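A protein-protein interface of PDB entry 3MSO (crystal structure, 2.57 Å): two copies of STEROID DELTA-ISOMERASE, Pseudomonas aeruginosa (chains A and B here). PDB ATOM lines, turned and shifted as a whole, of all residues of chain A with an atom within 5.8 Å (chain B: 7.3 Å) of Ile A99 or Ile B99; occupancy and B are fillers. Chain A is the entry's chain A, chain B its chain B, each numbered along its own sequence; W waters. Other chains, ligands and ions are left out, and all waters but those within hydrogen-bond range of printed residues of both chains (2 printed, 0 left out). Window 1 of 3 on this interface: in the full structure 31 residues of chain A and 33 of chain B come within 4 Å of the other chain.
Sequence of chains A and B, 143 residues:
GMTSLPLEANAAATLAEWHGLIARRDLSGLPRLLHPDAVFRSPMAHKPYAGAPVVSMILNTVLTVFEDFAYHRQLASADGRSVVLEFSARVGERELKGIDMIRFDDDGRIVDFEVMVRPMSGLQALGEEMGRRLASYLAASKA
OE2 of Glu A86 is in salt-bridge range of NZ of Lys A97 (2.7 Å).
N of Phe A87 is in hydrogen-bond range of O of Gly A98.
N of Met A101 lies within hydrogen-bond range of O of Glu A114 (2.8 Å).
N of Val B84 lies within hydrogen-bond range of O of Leu B75 (2.8 Å).
N of Phe B87 sits at hydrogen-bond distance from O of Gly B98, 2.8 Å away.
N of Met B101 lies within hydrogen-bond range of O of Glu B114 (2.8 Å).
Water W2 bridges O of Met A101 (2.6 Å) and NH2 of Arg B73 (3.0 Å).
Water W1 lies within hydrogen-bond range of the backbone NH of Val B117 (2.8 Å) and the backbone carbonyl oxygen of Val A117 (3.1 Å).
Val A84 touches Leu B75 (CG2 to CD1, 3.8 Å).
Glu A86 touches Met B101 (OE2 to CE, 3.5 Å).
Glu A86 touches Glu B114.
Ile B99 touches Ile A99 (CD1 to CG2, 3.8 Å).
Ile A99 touches Met B116.
OE2 of Glu B86 touches CE of Met A101 (3.4 Å).
Glu B86 touches Glu A114.
Val A115 touches Arg B118 (O to CD, 3.3 Å).
Ile B99 touches Met A116.
Met A116 touches Arg B118.
Printed residues of chain A within 4 Å of Ile B99: Ile A99 (3.8 Å) and Met A116 (3.98 Å).
Printed residues of chain A within 4 Å of Leu B75: Val A84 (3.8 Å).
Printed residues of chain A within 4 Å of Gly B98: Met A116.
Of the printed residues of chain B, Val A84 touches Leu B75.
Asp A100 touches none of the printed residues of chain B.
Leu A85 touches none of the printed residues of chain B.
The nearest residue of chain B that does not touch Ile A99 is Met B101 (4.1 Å).
The nearest printed residue of chain A that does not touch Ile B99 is Met A101 (4.05 Å).
Glu A86 touches Met B101, and with the chains exchanged Met A101 touches Glu B86.
Lys A97 touches Glu B114, and with the chains exchanged Glu A114 touches Lys B97.
Ile B99 touches its own counterpart, Ile A99.
Met B116 touches its own counterpart, Met A116.
Positions printed for both chains: 84, 85, 86, 87, 97, 98, 99, 100, 101, 114, 115, 116 and 117.
Of the 18 pairs that touch across the chains among the printed residues, 12 have their exchanged pair printed and touching as well.
Printed residues of chain A that touch a printed residue of chain B: Val A84, Glu A86, Lys A97, Gly A98, Ile A99, Met A101, Glu A114, Val A115 and Met A116.
Hydrophobic or aromatic side chains of chain B that line the printed part of chain A: Leu B75, Ile B99, Met B101 and Met B116.
Among the printed residues, Asp or Glu carboxylates within 4 Å of a Lys or Arg side-chain nitrogen of the other chain: Lys A97 with Glu B114 (3.1 Å), Glu A114 with Arg B73 (3.6 Å), Glu A114 with Lys B97 (3.0 Å) and Glu A114 with Arg B118 (3.2 Å).
The side-chain amino group (NZ) of Lys A97 lies within salt-bridge range of the side-chain carboxylate (OE2) of Glu B114 (3.1 Å).
SD of Met A101 lies close to NH2 of Arg B73, 3.8 Å away.
The side-chain carboxylate (OE1) of Glu A114 lies within salt-bridge range of the guanidinium group (NH2) of Arg B73 (3.6 Å).
The side-chain carboxylate (OE2) of Glu A114 is in salt-bridge range of the side-chain amino group (NZ) of Lys B97.
OE2 of Glu A114 lies within salt-bridge range of NH1 of Arg B118 (3.2 Å).
O of Met A116 lies close to SD of Met B116, 3.7 Å away.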
ATOM      1  N   VAL A  84     -29.709 -23.851 -23.289  1.00  0.00           N
ATOM      2  CA  VAL A  84     -29.522 -23.519 -24.703  1.00  0.00           C
ATOM      3  C   VAL A  84     -29.987 -24.758 -25.479  1.00  0.00           C
ATOM      4  O   VAL A  84     -29.502 -25.876 -25.237  1.00  0.00           O
ATOM      5  CB  VAL A  84     -28.103 -23.040 -25.104  1.00  0.00           C
ATOM      6  CG1 VAL A  84     -27.869 -23.190 -26.603  1.00  0.00           C
ATOM      7  CG2 VAL A  84     -27.890 -21.604 -24.689  1.00  0.00           C
ATOM      8  N   LEU A  85     -30.989 -24.561 -26.336  1.00  0.00           N
ATOM      9  CA  LEU A  85     -31.543 -25.615 -27.186  1.00  0.00           C
ATOM     10  C   LEU A  85     -31.130 -25.296 -28.607  1.00  0.00           C
ATOM     11  O   LEU A  85     -31.644 -24.344 -29.202  1.00  0.00           O
ATOM     12  CB  LEU A  85     -33.078 -25.733 -27.059  1.00  0.00           C
ATOM     13  CG  LEU A  85     -33.669 -25.744 -25.639  1.00  0.00           C
ATOM     14  CD1 LEU A  85     -35.167 -25.632 -25.666  1.00  0.00           C
ATOM     15  CD2 LEU A  85     -33.215 -26.958 -24.849  1.00  0.00           C
ATOM     16  N   GLU A  86     -30.122 -26.032 -29.111  1.00  0.00           N
ATOM     17  CA  GLU A  86     -29.600 -25.901 -30.472  1.00  0.00           C
ATOM     18  C   GLU A  86     -30.613 -26.506 -31.432  1.00  0.00           C
ATOM     19  O   GLU A  86     -31.120 -27.598 -31.173  1.00  0.00           O
ATOM     20  CB  GLU A  86     -28.241 -26.637 -30.597  1.00  0.00           C
ATOM     21  CG  GLU A  86     -27.698 -26.716 -32.017  1.00  0.00           C
ATOM     22  CD  GLU A  86     -26.550 -27.681 -32.232  1.00  0.00           C
ATOM     23  OE1 GLU A  86     -26.584 -28.808 -31.682  1.00  0.00           O
ATOM     24  OE2 GLU A  86     -25.632 -27.325 -33.000  1.00  0.00           O
ATOM     25  N   PHE A  87     -30.899 -25.818 -32.535  1.00  0.00           N
ATOM     26  CA  PHE A  87     -31.827 -26.341 -33.547  1.00  0.00           C
ATOM     27  C   PHE A  87     -31.361 -26.094 -34.976  1.00  0.00           C
ATOM     28  O   PHE A  87     -30.569 -25.186 -35.251  1.00  0.00           O
ATOM     29  CB  PHE A  87     -33.268 -25.789 -33.344  1.00  0.00           C
ATOM     30  CG  PHE A  87     -33.444 -24.299 -33.548  1.00  0.00           C
ATOM     31  CD1 PHE A  87     -33.618 -23.766 -34.824  1.00  0.00           C
ATOM     32  CD2 PHE A  87     -33.472 -23.430 -32.462  1.00  0.00           C
ATOM     33  CE1 PHE A  87     -33.791 -22.382 -35.010  1.00  0.00           C
ATOM     34  CE2 PHE A  87     -33.634 -22.035 -32.652  1.00  0.00           C
ATOM     35  CZ  PHE A  87     -33.771 -21.522 -33.920  1.00  0.00           C
ATOM     36  N   LYS A  97     -29.606 -22.508 -38.899  1.00  0.00           N
ATOM     37  CA  LYS A  97     -29.123 -23.060 -37.650  1.00  0.00           C
ATOM     38  C   LYS A  97     -29.425 -22.022 -36.582  1.00  0.00           C
ATOM     39  O   LYS A  97     -29.339 -20.818 -36.848  1.00  0.00           O
ATOM     40  CB  LYS A  97     -27.621 -23.244 -37.804  1.00  0.00           C
ATOM     41  CG  LYS A  97     -27.050 -24.317 -36.970  1.00  0.00           C
ATOM     42  CD  LYS A  97     -27.495 -25.714 -37.323  1.00  0.00           C
ATOM     43  CE  LYS A  97     -27.293 -26.468 -36.033  1.00  0.00           C
ATOM     44  NZ  LYS A  97     -25.910 -26.292 -35.491  1.00  0.00           N
ATOM     45  N   GLY A  98     -29.811 -22.473 -35.402  1.00  0.00           N
ATOM     46  CA  GLY A  98     -30.160 -21.536 -34.342  1.00  0.00           C
ATOM     47  C   GLY A  98     -30.119 -22.071 -32.933  1.00  0.00           C
ATOM     48  O   GLY A  98     -29.888 -23.271 -32.710  1.00  0.00           O
ATOM     49  N   ILE A  99     -30.360 -21.164 -31.971  1.00  0.00           N
ATOM     50  CA  ILE A  99     -30.437 -21.474 -30.547  1.00  0.00           C
ATOM     51  C   ILE A  99     -31.610 -20.796 -29.854  1.00  0.00           C
ATOM     52  O   ILE A  99     -31.919 -19.647 -30.144  1.00  0.00           O
ATOM     53  CB  ILE A  99     -29.108 -21.208 -29.754  1.00  0.00           C
ATOM     54  CG1 ILE A  99     -28.663 -19.718 -29.800  1.00  0.00           C
ATOM     55  CG2 ILE A  99     -27.990 -22.170 -30.151  1.00  0.00           C
ATOM     56  CD1 ILE A  99     -28.066 -19.164 -28.457  1.00  0.00           C
ATOM     57  N   ASP A 100     -32.254 -21.506 -28.927  1.00  0.00           N
ATOM     58  CA  ASP A 100     -33.258 -20.955 -28.025  1.00  0.00           C
ATOM     59  C   ASP A 100     -32.482 -20.907 -26.718  1.00  0.00           C
ATOM     60  O   ASP A 100     -32.076 -21.963 -26.251  1.00  0.00           O
ATOM     61  CB  ASP A 100     -34.474 -21.890 -27.855  1.00  0.00           C
ATOM     62  CG  ASP A 100     -35.402 -21.955 -29.035  1.00  0.00           C
ATOM     63  OD1 ASP A 100     -35.605 -20.908 -29.679  1.00  0.00           O
ATOM     64  OD2 ASP A 100     -35.972 -23.043 -29.279  1.00  0.00           O
ATOM     65  N   MET A 101     -32.168 -19.696 -26.204  1.00  0.00           N
ATOM     66  CA  MET A 101     -31.448 -19.527 -24.950  1.00  0.00           C
ATOM     67  C   MET A 101     -32.448 -19.025 -23.926  1.00  0.00           C
ATOM     68  O   MET A 101     -32.787 -17.839 -23.918  1.00  0.00           O
ATOM     69  CB  MET A 101     -30.211 -18.607 -25.091  1.00  0.00           C
ATOM     70  CG  MET A 101     -29.421 -18.441 -23.763  1.00  0.00           C
ATOM     71  SD  MET A 101     -27.534 -18.132 -24.039  1.00  0.00           S
ATOM     72  CE  MET A 101     -27.630 -16.537 -25.142  1.00  0.00           C
ATOM     73  N   GLU A 114     -34.133 -15.749 -25.552  1.00  0.00           N
ATOM     74  CA  GLU A 114     -33.269 -15.150 -26.556  1.00  0.00           C
ATOM     75  C   GLU A 114     -32.991 -16.136 -27.702  1.00  0.00           C
ATOM     76  O   GLU A 114     -32.556 -17.268 -27.479  1.00  0.00           O
ATOM     77  CB  GLU A 114     -31.983 -14.705 -25.863  1.00  0.00           C
ATOM     78  CG  GLU A 114     -31.026 -13.906 -26.709  1.00  0.00           C
ATOM     79  CD  GLU A 114     -29.841 -13.393 -25.917  1.00  0.00           C
ATOM     80  OE1 GLU A 114     -29.759 -13.653 -24.692  1.00  0.00           O
ATOM     81  OE2 GLU A 114     -29.000 -12.698 -26.525  1.00  0.00           O
ATOM     82  N   VAL A 115     -33.265 -15.703 -28.925  1.00  0.00           N
ATOM     83  CA  VAL A 115     -33.058 -16.521 -30.115  1.00  0.00           C
ATOM     84  C   VAL A 115     -31.940 -15.909 -30.979  1.00  0.00           C
ATOM     85  O   VAL A 115     -31.841 -14.684 -31.090  1.00  0.00           O
ATOM     86  CB  VAL A 115     -34.380 -16.692 -30.926  1.00  0.00           C
ATOM     87  CG1 VAL A 115     -34.166 -17.516 -32.207  1.00  0.00           C
ATOM     88  CG2 VAL A 115     -35.489 -17.299 -30.055  1.00  0.00           C
ATOM     89  N   MET A 116     -31.079 -16.782 -31.553  1.00  0.00           N
ATOM     90  CA  MET A 116     -30.018 -16.417 -32.506  1.00  0.00           C
ATOM     91  C   MET A 116     -30.104 -17.393 -33.649  1.00  0.00           C
ATOM     92  O   MET A 116     -30.400 -18.570 -33.447  1.00  0.00           O
ATOM     93  CB  MET A 116     -28.600 -16.455 -31.893  1.00  0.00           C
ATOM     94  CG  MET A 116     -28.452 -15.591 -30.659  1.00  0.00           C
ATOM     95  SD  MET A 116     -26.638 -15.412 -30.156  1.00  0.00           S
ATOM     96  CE  MET A 116     -26.867 -14.731 -28.418  1.00  0.00           C
ATOM     97  N   VAL A 117     -29.878 -16.900 -34.840  1.00  0.00           N
ATOM     98  CA  VAL A 117     -29.947 -17.674 -36.074  1.00  0.00           C
ATOM     99  C   VAL A 117     -28.695 -17.360 -36.897  1.00  0.00           C
ATOM    100  O   VAL A 117     -28.129 -16.266 -36.794  1.00  0.00           O
ATOM    101  CB  VAL A 117     -31.305 -17.387 -36.818  1.00  0.00           C
ATOM    102  CG1 VAL A 117     -31.233 -17.679 -38.303  1.00  0.00           C
ATOM    103  CG2 VAL A 117     -32.460 -18.166 -36.175  1.00  0.00           C
ATOM    104  N   PRO B  43     -20.968 -17.056 -38.403  1.00  0.00           N
ATOM    105  CA  PRO B  43     -22.332 -16.520 -38.259  1.00  0.00           C
ATOM    106  C   PRO B  43     -22.837 -15.911 -39.573  1.00  0.00           C
ATOM    107  O   PRO B  43     -24.033 -15.683 -39.718  1.00  0.00           O
ATOM    108  CB  PRO B  43     -22.165 -15.437 -37.184  1.00  0.00           C
ATOM    109  CG  PRO B  43     -20.737 -15.012 -37.282  1.00  0.00           C
ATOM    110  CD  PRO B  43     -19.978 -16.235 -37.661  1.00  0.00           C
ATOM    111  N   TYR B  71     -17.623 -12.244 -21.682  1.00  0.00           N
ATOM    112  CA  TYR B  71     -18.341 -13.520 -21.569  1.00  0.00           C
ATOM    113  C   TYR B  71     -19.374 -13.415 -20.456  1.00  0.00           C
ATOM    114  O   TYR B  71     -19.175 -12.673 -19.498  1.00  0.00           O
ATOM    115  CB  TYR B  71     -17.378 -14.682 -21.287  1.00  0.00           C
ATOM    116  CG  TYR B  71     -16.723 -15.252 -22.533  1.00  0.00           C
ATOM    117  CD1 TYR B  71     -17.487 -15.619 -23.646  1.00  0.00           C
ATOM    118  CD2 TYR B  71     -15.352 -15.469 -22.584  1.00  0.00           C
ATOM    119  CE1 TYR B  71     -16.895 -16.186 -24.773  1.00  0.00           C
ATOM    120  CE2 TYR B  71     -14.753 -16.048 -23.701  1.00  0.00           C
ATOM    121  CZ  TYR B  71     -15.530 -16.416 -24.787  1.00  0.00           C
ATOM    122  OH  TYR B  71     -14.940 -16.964 -25.894  1.00  0.00           O
ATOM    123  N   ARG B  73     -23.032 -16.070 -19.590  1.00  0.00           N
ATOM    124  CA  ARG B  73     -23.398 -17.439 -19.237  1.00  0.00           C
ATOM    125  C   ARG B  73     -22.561 -18.460 -19.977  1.00  0.00           C
ATOM    126  O   ARG B  73     -22.184 -18.266 -21.143  1.00  0.00           O
ATOM    127  CB  ARG B  73     -24.893 -17.722 -19.533  1.00  0.00           C
ATOM    128  CG  ARG B  73     -25.852 -17.093 -18.530  1.00  0.00           C
ATOM    129  CD  ARG B  73     -27.284 -17.281 -18.957  1.00  0.00           C
ATOM    130  NE  ARG B  73     -27.612 -16.467 -20.131  1.00  0.00           N
ATOM    131  CZ  ARG B  73     -28.833 -16.360 -20.635  1.00  0.00           C
ATOM    132  NH1 ARG B  73     -29.849 -17.003 -20.072  1.00  0.00           N
ATOM    133  NH2 ARG B  73     -29.054 -15.597 -21.691  1.00  0.00           N
ATOM    134  N   LEU B  75     -22.736 -22.641 -20.597  1.00  0.00           N
ATOM    135  CA  LEU B  75     -23.602 -23.800 -20.538  1.00  0.00           C
ATOM    136  C   LEU B  75     -22.913 -25.011 -21.148  1.00  0.00           C
ATOM    137  O   LEU B  75     -22.253 -24.902 -22.182  1.00  0.00           O
ATOM    138  CB  LEU B  75     -24.913 -23.497 -21.309  1.00  0.00           C
ATOM    139  CG  LEU B  75     -25.636 -22.164 -20.982  1.00  0.00           C
ATOM    140  CD1 LEU B  75     -25.291 -21.075 -22.004  1.00  0.00           C
ATOM    141  CD2 LEU B  75     -27.126 -22.364 -20.871  1.00  0.00           C
ATOM    142  N   VAL B  83     -19.868 -26.991 -25.174  1.00  0.00           N
ATOM    143  CA  VAL B  83     -20.026 -25.795 -24.373  1.00  0.00           C
ATOM    144  C   VAL B  83     -20.596 -24.657 -25.216  1.00  0.00           C
ATOM    145  O   VAL B  83     -20.332 -24.578 -26.422  1.00  0.00           O
ATOM    146  CB  VAL B  83     -18.665 -25.434 -23.705  1.00  0.00           C
ATOM    147  CG1 VAL B  83     -17.706 -24.709 -24.652  1.00  0.00           C
ATOM    148  CG2 VAL B  83     -18.859 -24.647 -22.417  1.00  0.00           C
ATOM    149  N   VAL B  84     -21.401 -23.804 -24.593  1.00  0.00           N
ATOM    150  CA  VAL B  84     -21.890 -22.567 -25.194  1.00  0.00           C
ATOM    151  C   VAL B  84     -21.406 -21.440 -24.283  1.00  0.00           C
ATOM    152  O   VAL B  84     -21.686 -21.448 -23.072  1.00  0.00           O
ATOM    153  CB  VAL B  84     -23.419 -22.516 -25.469  1.00  0.00           C
ATOM    154  CG1 VAL B  84     -23.912 -21.071 -25.610  1.00  0.00           C
ATOM    155  CG2 VAL B  84     -23.772 -23.324 -26.711  1.00  0.00           C
ATOM    156  N   LEU B  85     -20.617 -20.527 -24.865  1.00  0.00           N
ATOM    157  CA  LEU B  85     -20.090 -19.352 -24.165  1.00  0.00           C
ATOM    158  C   LEU B  85     -20.809 -18.133 -24.709  1.00  0.00           C
ATOM    159  O   LEU B  85     -20.569 -17.737 -25.858  1.00  0.00           O
ATOM    160  CB  LEU B  85     -18.554 -19.206 -24.329  1.00  0.00           C
ATOM    161  CG  LEU B  85     -17.715 -20.463 -24.114  1.00  0.00           C
ATOM    162  CD1 LEU B  85     -16.289 -20.235 -24.535  1.00  0.00           C
ATOM    163  CD2 LEU B  85     -17.833 -20.975 -22.669  1.00  0.00           C
ATOM    164  N   GLU B  86     -21.758 -17.606 -23.918  1.00  0.00           N
ATOM    165  CA  GLU B  86     -22.555 -16.423 -24.255  1.00  0.00           C
ATOM    166  C   GLU B  86     -21.667 -15.195 -24.087  1.00  0.00           C
ATOM    167  O   GLU B  86     -20.961 -15.088 -23.072  1.00  0.00           O
ATOM    168  CB  GLU B  86     -23.780 -16.321 -23.319  1.00  0.00           C
ATOM    169  CG  GLU B  86     -24.555 -15.023 -23.452  1.00  0.00           C
ATOM    170  CD  GLU B  86     -25.576 -14.751 -22.375  1.00  0.00           C
ATOM    171  OE1 GLU B  86     -25.274 -14.959 -21.180  1.00  0.00           O
ATOM    172  OE2 GLU B  86     -26.672 -14.276 -22.732  1.00  0.00           O
ATOM    173  N   PHE B  87     -21.713 -14.260 -25.058  1.00  0.00           N
ATOM    174  CA  PHE B  87     -20.945 -13.029 -24.972  1.00  0.00           C
ATOM    175  C   PHE B  87     -21.707 -11.803 -25.434  1.00  0.00           C
ATOM    176  O   PHE B  87     -22.671 -11.900 -26.211  1.00  0.00           O
ATOM    177  CB  PHE B  87     -19.590 -13.142 -25.728  1.00  0.00           C
ATOM    178  CG  PHE B  87     -19.672 -13.306 -27.237  1.00  0.00           C
ATOM    179  CD1 PHE B  87     -19.833 -12.199 -28.071  1.00  0.00           C
ATOM    180  CD2 PHE B  87     -19.559 -14.564 -27.824  1.00  0.00           C
ATOM    181  CE1 PHE B  87     -19.905 -12.349 -29.457  1.00  0.00           C
ATOM    182  CE2 PHE B  87     -19.640 -14.712 -29.222  1.00  0.00           C
ATOM    183  CZ  PHE B  87     -19.834 -13.606 -30.020  1.00  0.00           C
ATOM    184  N   SER B  88     -21.218 -10.636 -24.997  1.00  0.00           N
ATOM    185  CA  SER B  88     -21.628  -9.307 -25.430  1.00  0.00           C
ATOM    186  C   SER B  88     -20.376  -8.710 -26.047  1.00  0.00           C
ATOM    187  O   SER B  88     -19.269  -9.080 -25.671  1.00  0.00           O
ATOM    188  CB  SER B  88     -22.086  -8.463 -24.254  1.00  0.00           C
ATOM    189  OG  SER B  88     -21.101  -8.431 -23.235  1.00  0.00           O
ATOM    190  N   LEU B  96     -23.692  -5.732 -29.802  1.00  0.00           N
ATOM    191  CA  LEU B  96     -24.119  -7.071 -30.201  1.00  0.00           C
ATOM    192  C   LEU B  96     -24.095  -8.114 -29.084  1.00  0.00           C
ATOM    193  O   LEU B  96     -23.513  -7.921 -28.015  1.00  0.00           O
ATOM    194  CB  LEU B  96     -23.456  -7.573 -31.506  1.00  0.00           C
ATOM    195  CG  LEU B  96     -21.956  -7.851 -31.470  1.00  0.00           C
ATOM    196  CD1 LEU B  96     -21.620  -9.275 -30.916  1.00  0.00           C
ATOM    197  CD2 LEU B  96     -21.353  -7.680 -32.828  1.00  0.00           C
ATOM    198  N   LYS B  97     -24.708  -9.243 -29.390  1.00  0.00           N
ATOM    199  CA  LYS B  97     -24.852 -10.380 -28.505  1.00  0.00           C
ATOM    200  C   LYS B  97     -24.507 -11.620 -29.313  1.00  0.00           C
ATOM    201  O   LYS B  97     -24.822 -11.676 -30.516  1.00  0.00           O
ATOM    202  CB  LYS B  97     -26.318 -10.414 -28.085  1.00  0.00           C
ATOM    203  CG  LYS B  97     -26.567 -11.010 -26.760  1.00  0.00           C
ATOM    204  CD  LYS B  97     -25.992 -10.262 -25.580  1.00  0.00           C
ATOM    205  CE  LYS B  97     -25.801 -11.337 -24.537  1.00  0.00           C
ATOM    206  NZ  LYS B  97     -27.046 -12.161 -24.363  1.00  0.00           N
ATOM    207  N   GLY B  98     -23.825 -12.571 -28.686  1.00  0.00           N
ATOM    208  CA  GLY B  98     -23.415 -13.769 -29.404  1.00  0.00           C
ATOM    209  C   GLY B  98     -23.108 -14.985 -28.570  1.00  0.00           C
ATOM    210  O   GLY B  98     -23.113 -14.924 -27.338  1.00  0.00           O
ATOM    211  N   ILE B  99     -22.822 -16.107 -29.263  1.00  0.00           N
ATOM    212  CA  ILE B  99     -22.423 -17.375 -28.655  1.00  0.00           C
ATOM    213  C   ILE B  99     -21.254 -18.027 -29.377  1.00  0.00           C
ATOM    214  O   ILE B  99     -21.188 -18.002 -30.593  1.00  0.00           O
ATOM    215  CB  ILE B  99     -23.587 -18.404 -28.462  1.00  0.00           C
ATOM    216  CG1 ILE B  99     -24.253 -18.818 -29.796  1.00  0.00           C
ATOM    217  CG2 ILE B  99     -24.596 -17.945 -27.424  1.00  0.00           C
ATOM    218  CD1 ILE B  99     -24.664 -20.335 -29.877  1.00  0.00           C
ATOM    219  N   ASP B 100     -20.339 -18.637 -28.616  1.00  0.00           N
ATOM    220  CA  ASP B 100     -19.271 -19.487 -29.144  1.00  0.00           C
ATOM    221  C   ASP B 100     -19.784 -20.868 -28.739  1.00  0.00           C
ATOM    222  O   ASP B 100     -19.944 -21.112 -27.535  1.00  0.00           O
ATOM    223  CB  ASP B 100     -17.910 -19.220 -28.456  1.00  0.00           C
ATOM    224  CG  ASP B 100     -17.248 -17.912 -28.840  1.00  0.00           C
ATOM    225  OD1 ASP B 100     -17.351 -17.523 -30.018  1.00  0.00           O
ATOM    226  OD2 ASP B 100     -16.576 -17.304 -27.972  1.00  0.00           O
ATOM    227  N   MET B 101     -20.167 -21.710 -29.713  1.00  0.00           N
ATOM    228  CA  MET B 101     -20.639 -23.067 -29.434  1.00  0.00           C
ATOM    229  C   MET B 101     -19.529 -24.030 -29.848  1.00  0.00           C
ATOM    230  O   MET B 101     -19.352 -24.313 -31.030  1.00  0.00           O
ATOM    231  CB  MET B 101     -21.985 -23.380 -30.102  1.00  0.00           C
ATOM    232  CG  MET B 101     -22.503 -24.804 -29.798  1.00  0.00           C
ATOM    233  SD  MET B 101     -24.455 -24.918 -29.834  1.00  0.00           S
ATOM    234  CE  MET B 101     -24.797 -24.266 -31.591  1.00  0.00           C
ATOM    235  N   ILE B 102     -18.765 -24.488 -28.853  1.00  0.00           N
ATOM    236  CA  ILE B 102     -17.587 -25.332 -29.027  1.00  0.00           C
ATOM    237  C   ILE B 102     -17.855 -26.804 -28.692  1.00  0.00           C
ATOM    238  O   ILE B 102     -18.337 -27.112 -27.592  1.00  0.00           O
ATOM    239  CB  ILE B 102     -16.378 -24.774 -28.175  1.00  0.00           C
ATOM    240  CG1 ILE B 102     -16.242 -23.213 -28.276  1.00  0.00           C
ATOM    241  CG2 ILE B 102     -15.061 -25.515 -28.491  1.00  0.00           C
ATOM    242  CD1 ILE B 102     -15.314 -22.587 -27.314  1.00  0.00           C
ATOM    243  N   PHE B 113     -16.319 -25.260 -34.051  1.00  0.00           N
ATOM    244  CA  PHE B 113     -16.460 -23.965 -33.426  1.00  0.00           C
ATOM    245  C   PHE B 113     -17.475 -23.205 -34.252  1.00  0.00           C
ATOM    246  O   PHE B 113     -17.182 -22.781 -35.375  1.00  0.00           O
ATOM    247  CB  PHE B 113     -15.121 -23.230 -33.406  1.00  0.00           C
ATOM    248  CG  PHE B 113     -15.011 -22.143 -32.361  1.00  0.00           C
ATOM    249  CD1 PHE B 113     -15.858 -21.037 -32.388  1.00  0.00           C
ATOM    250  CD2 PHE B 113     -14.011 -22.184 -31.395  1.00  0.00           C
ATOM    251  CE1 PHE B 113     -15.735 -20.017 -31.444  1.00  0.00           C
ATOM    252  CE2 PHE B 113     -13.892 -21.161 -30.448  1.00  0.00           C
ATOM    253  CZ  PHE B 113     -14.749 -20.079 -30.488  1.00  0.00           C
ATOM    254  N   GLU B 114     -18.684 -23.053 -33.692  1.00  0.00           N
ATOM    255  CA  GLU B 114     -19.820 -22.397 -34.323  1.00  0.00           C
ATOM    256  C   GLU B 114     -20.169 -21.105 -33.606  1.00  0.00           C
ATOM    257  O   GLU B 114     -20.383 -21.101 -32.395  1.00  0.00           O
ATOM    258  CB  GLU B 114     -20.985 -23.370 -34.336  1.00  0.00           C
ATOM    259  CG  GLU B 114     -22.199 -22.925 -35.111  1.00  0.00           C
ATOM    260  CD  GLU B 114     -23.267 -23.994 -35.229  1.00  0.00           C
ATOM    261  OE1 GLU B 114     -23.075 -25.107 -34.688  1.00  0.00           O
ATOM    262  OE2 GLU B 114     -24.311 -23.706 -35.853  1.00  0.00           O
ATOM    263  N   VAL B 115     -20.202 -19.998 -34.356  1.00  0.00           N
ATOM    264  CA  VAL B 115     -20.527 -18.676 -33.804  1.00  0.00           C
ATOM    265  C   VAL B 115     -21.878 -18.192 -34.348  1.00  0.00           C
ATOM    266  O   VAL B 115     -22.174 -18.407 -35.519  1.00  0.00           O
ATOM    267  CB  VAL B 115     -19.383 -17.649 -34.082  1.00  0.00           C
ATOM    268  CG1 VAL B 115     -19.713 -16.262 -33.526  1.00  0.00           C
ATOM    269  CG2 VAL B 115     -18.050 -18.141 -33.528  1.00  0.00           C
ATOM    270  N   MET B 116     -22.702 -17.573 -33.484  1.00  0.00           N
ATOM    271  CA  MET B 116     -23.975 -16.913 -33.851  1.00  0.00           C
ATOM    272  C   MET B 116     -23.959 -15.525 -33.188  1.00  0.00           C
ATOM    273  O   MET B 116     -23.457 -15.360 -32.072  1.00  0.00           O
ATOM    274  CB  MET B 116     -25.216 -17.673 -33.386  1.00  0.00           C
ATOM    275  CG  MET B 116     -25.257 -19.111 -33.854  1.00  0.00           C
ATOM    276  SD  MET B 116     -26.987 -19.892 -33.538  1.00  0.00           S
ATOM    277  CE  MET B 116     -26.472 -21.743 -33.828  1.00  0.00           C
ATOM    278  N   VAL B 117     -24.479 -14.538 -33.896  1.00  0.00           N
ATOM    279  CA  VAL B 117     -24.529 -13.156 -33.441  1.00  0.00           C
ATOM    280  C   VAL B 117     -25.944 -12.637 -33.692  1.00  0.00           C
ATOM    281  O   VAL B 117     -26.616 -13.100 -34.617  1.00  0.00           O
ATOM    282  CB  VAL B 117     -23.390 -12.317 -34.130  1.00  0.00           C
ATOM    283  CG1 VAL B 117     -23.702 -10.818 -34.165  1.00  0.00           C
ATOM    284  CG2 VAL B 117     -22.030 -12.569 -33.460  1.00  0.00           C
ATOM    285  N   ARG B 118     -26.415 -11.743 -32.815  1.00  0.00           N
ATOM    286  CA  ARG B 118     -27.695 -11.031 -32.911  1.00  0.00           C
ATOM    287  C   ARG B 118     -27.499  -9.583 -32.382  1.00  0.00           C
ATOM    288  O   ARG B 118     -26.629  -9.385 -31.520  1.00  0.00           O
ATOM    289  CB  ARG B 118     -28.826 -11.775 -32.183  1.00  0.00           C
ATOM    290  CG  ARG B 118     -28.656 -11.885 -30.671  1.00  0.00           C
ATOM    291  CD  ARG B 118     -29.976 -12.235 -30.008  1.00  0.00           C
ATOM    292  NE  ARG B 118     -30.911 -11.108 -30.040  1.00  0.00           N
ATOM    293  CZ  ARG B 118     -30.950 -10.153 -29.120  1.00  0.00           C
ATOM    294  NH1 ARG B 118     -30.125 -10.189 -28.082  1.00  0.00           N
ATOM    295  NH2 ARG B 118     -31.821  -9.160 -29.224  1.00  0.00           N
HETATM  296  O   HOH W   1     -25.284 -15.210 -36.483  1.00  0.00           O
HETATM  297  O   HOH W   2     -31.939 -16.029 -22.195  1.00  0.00           O
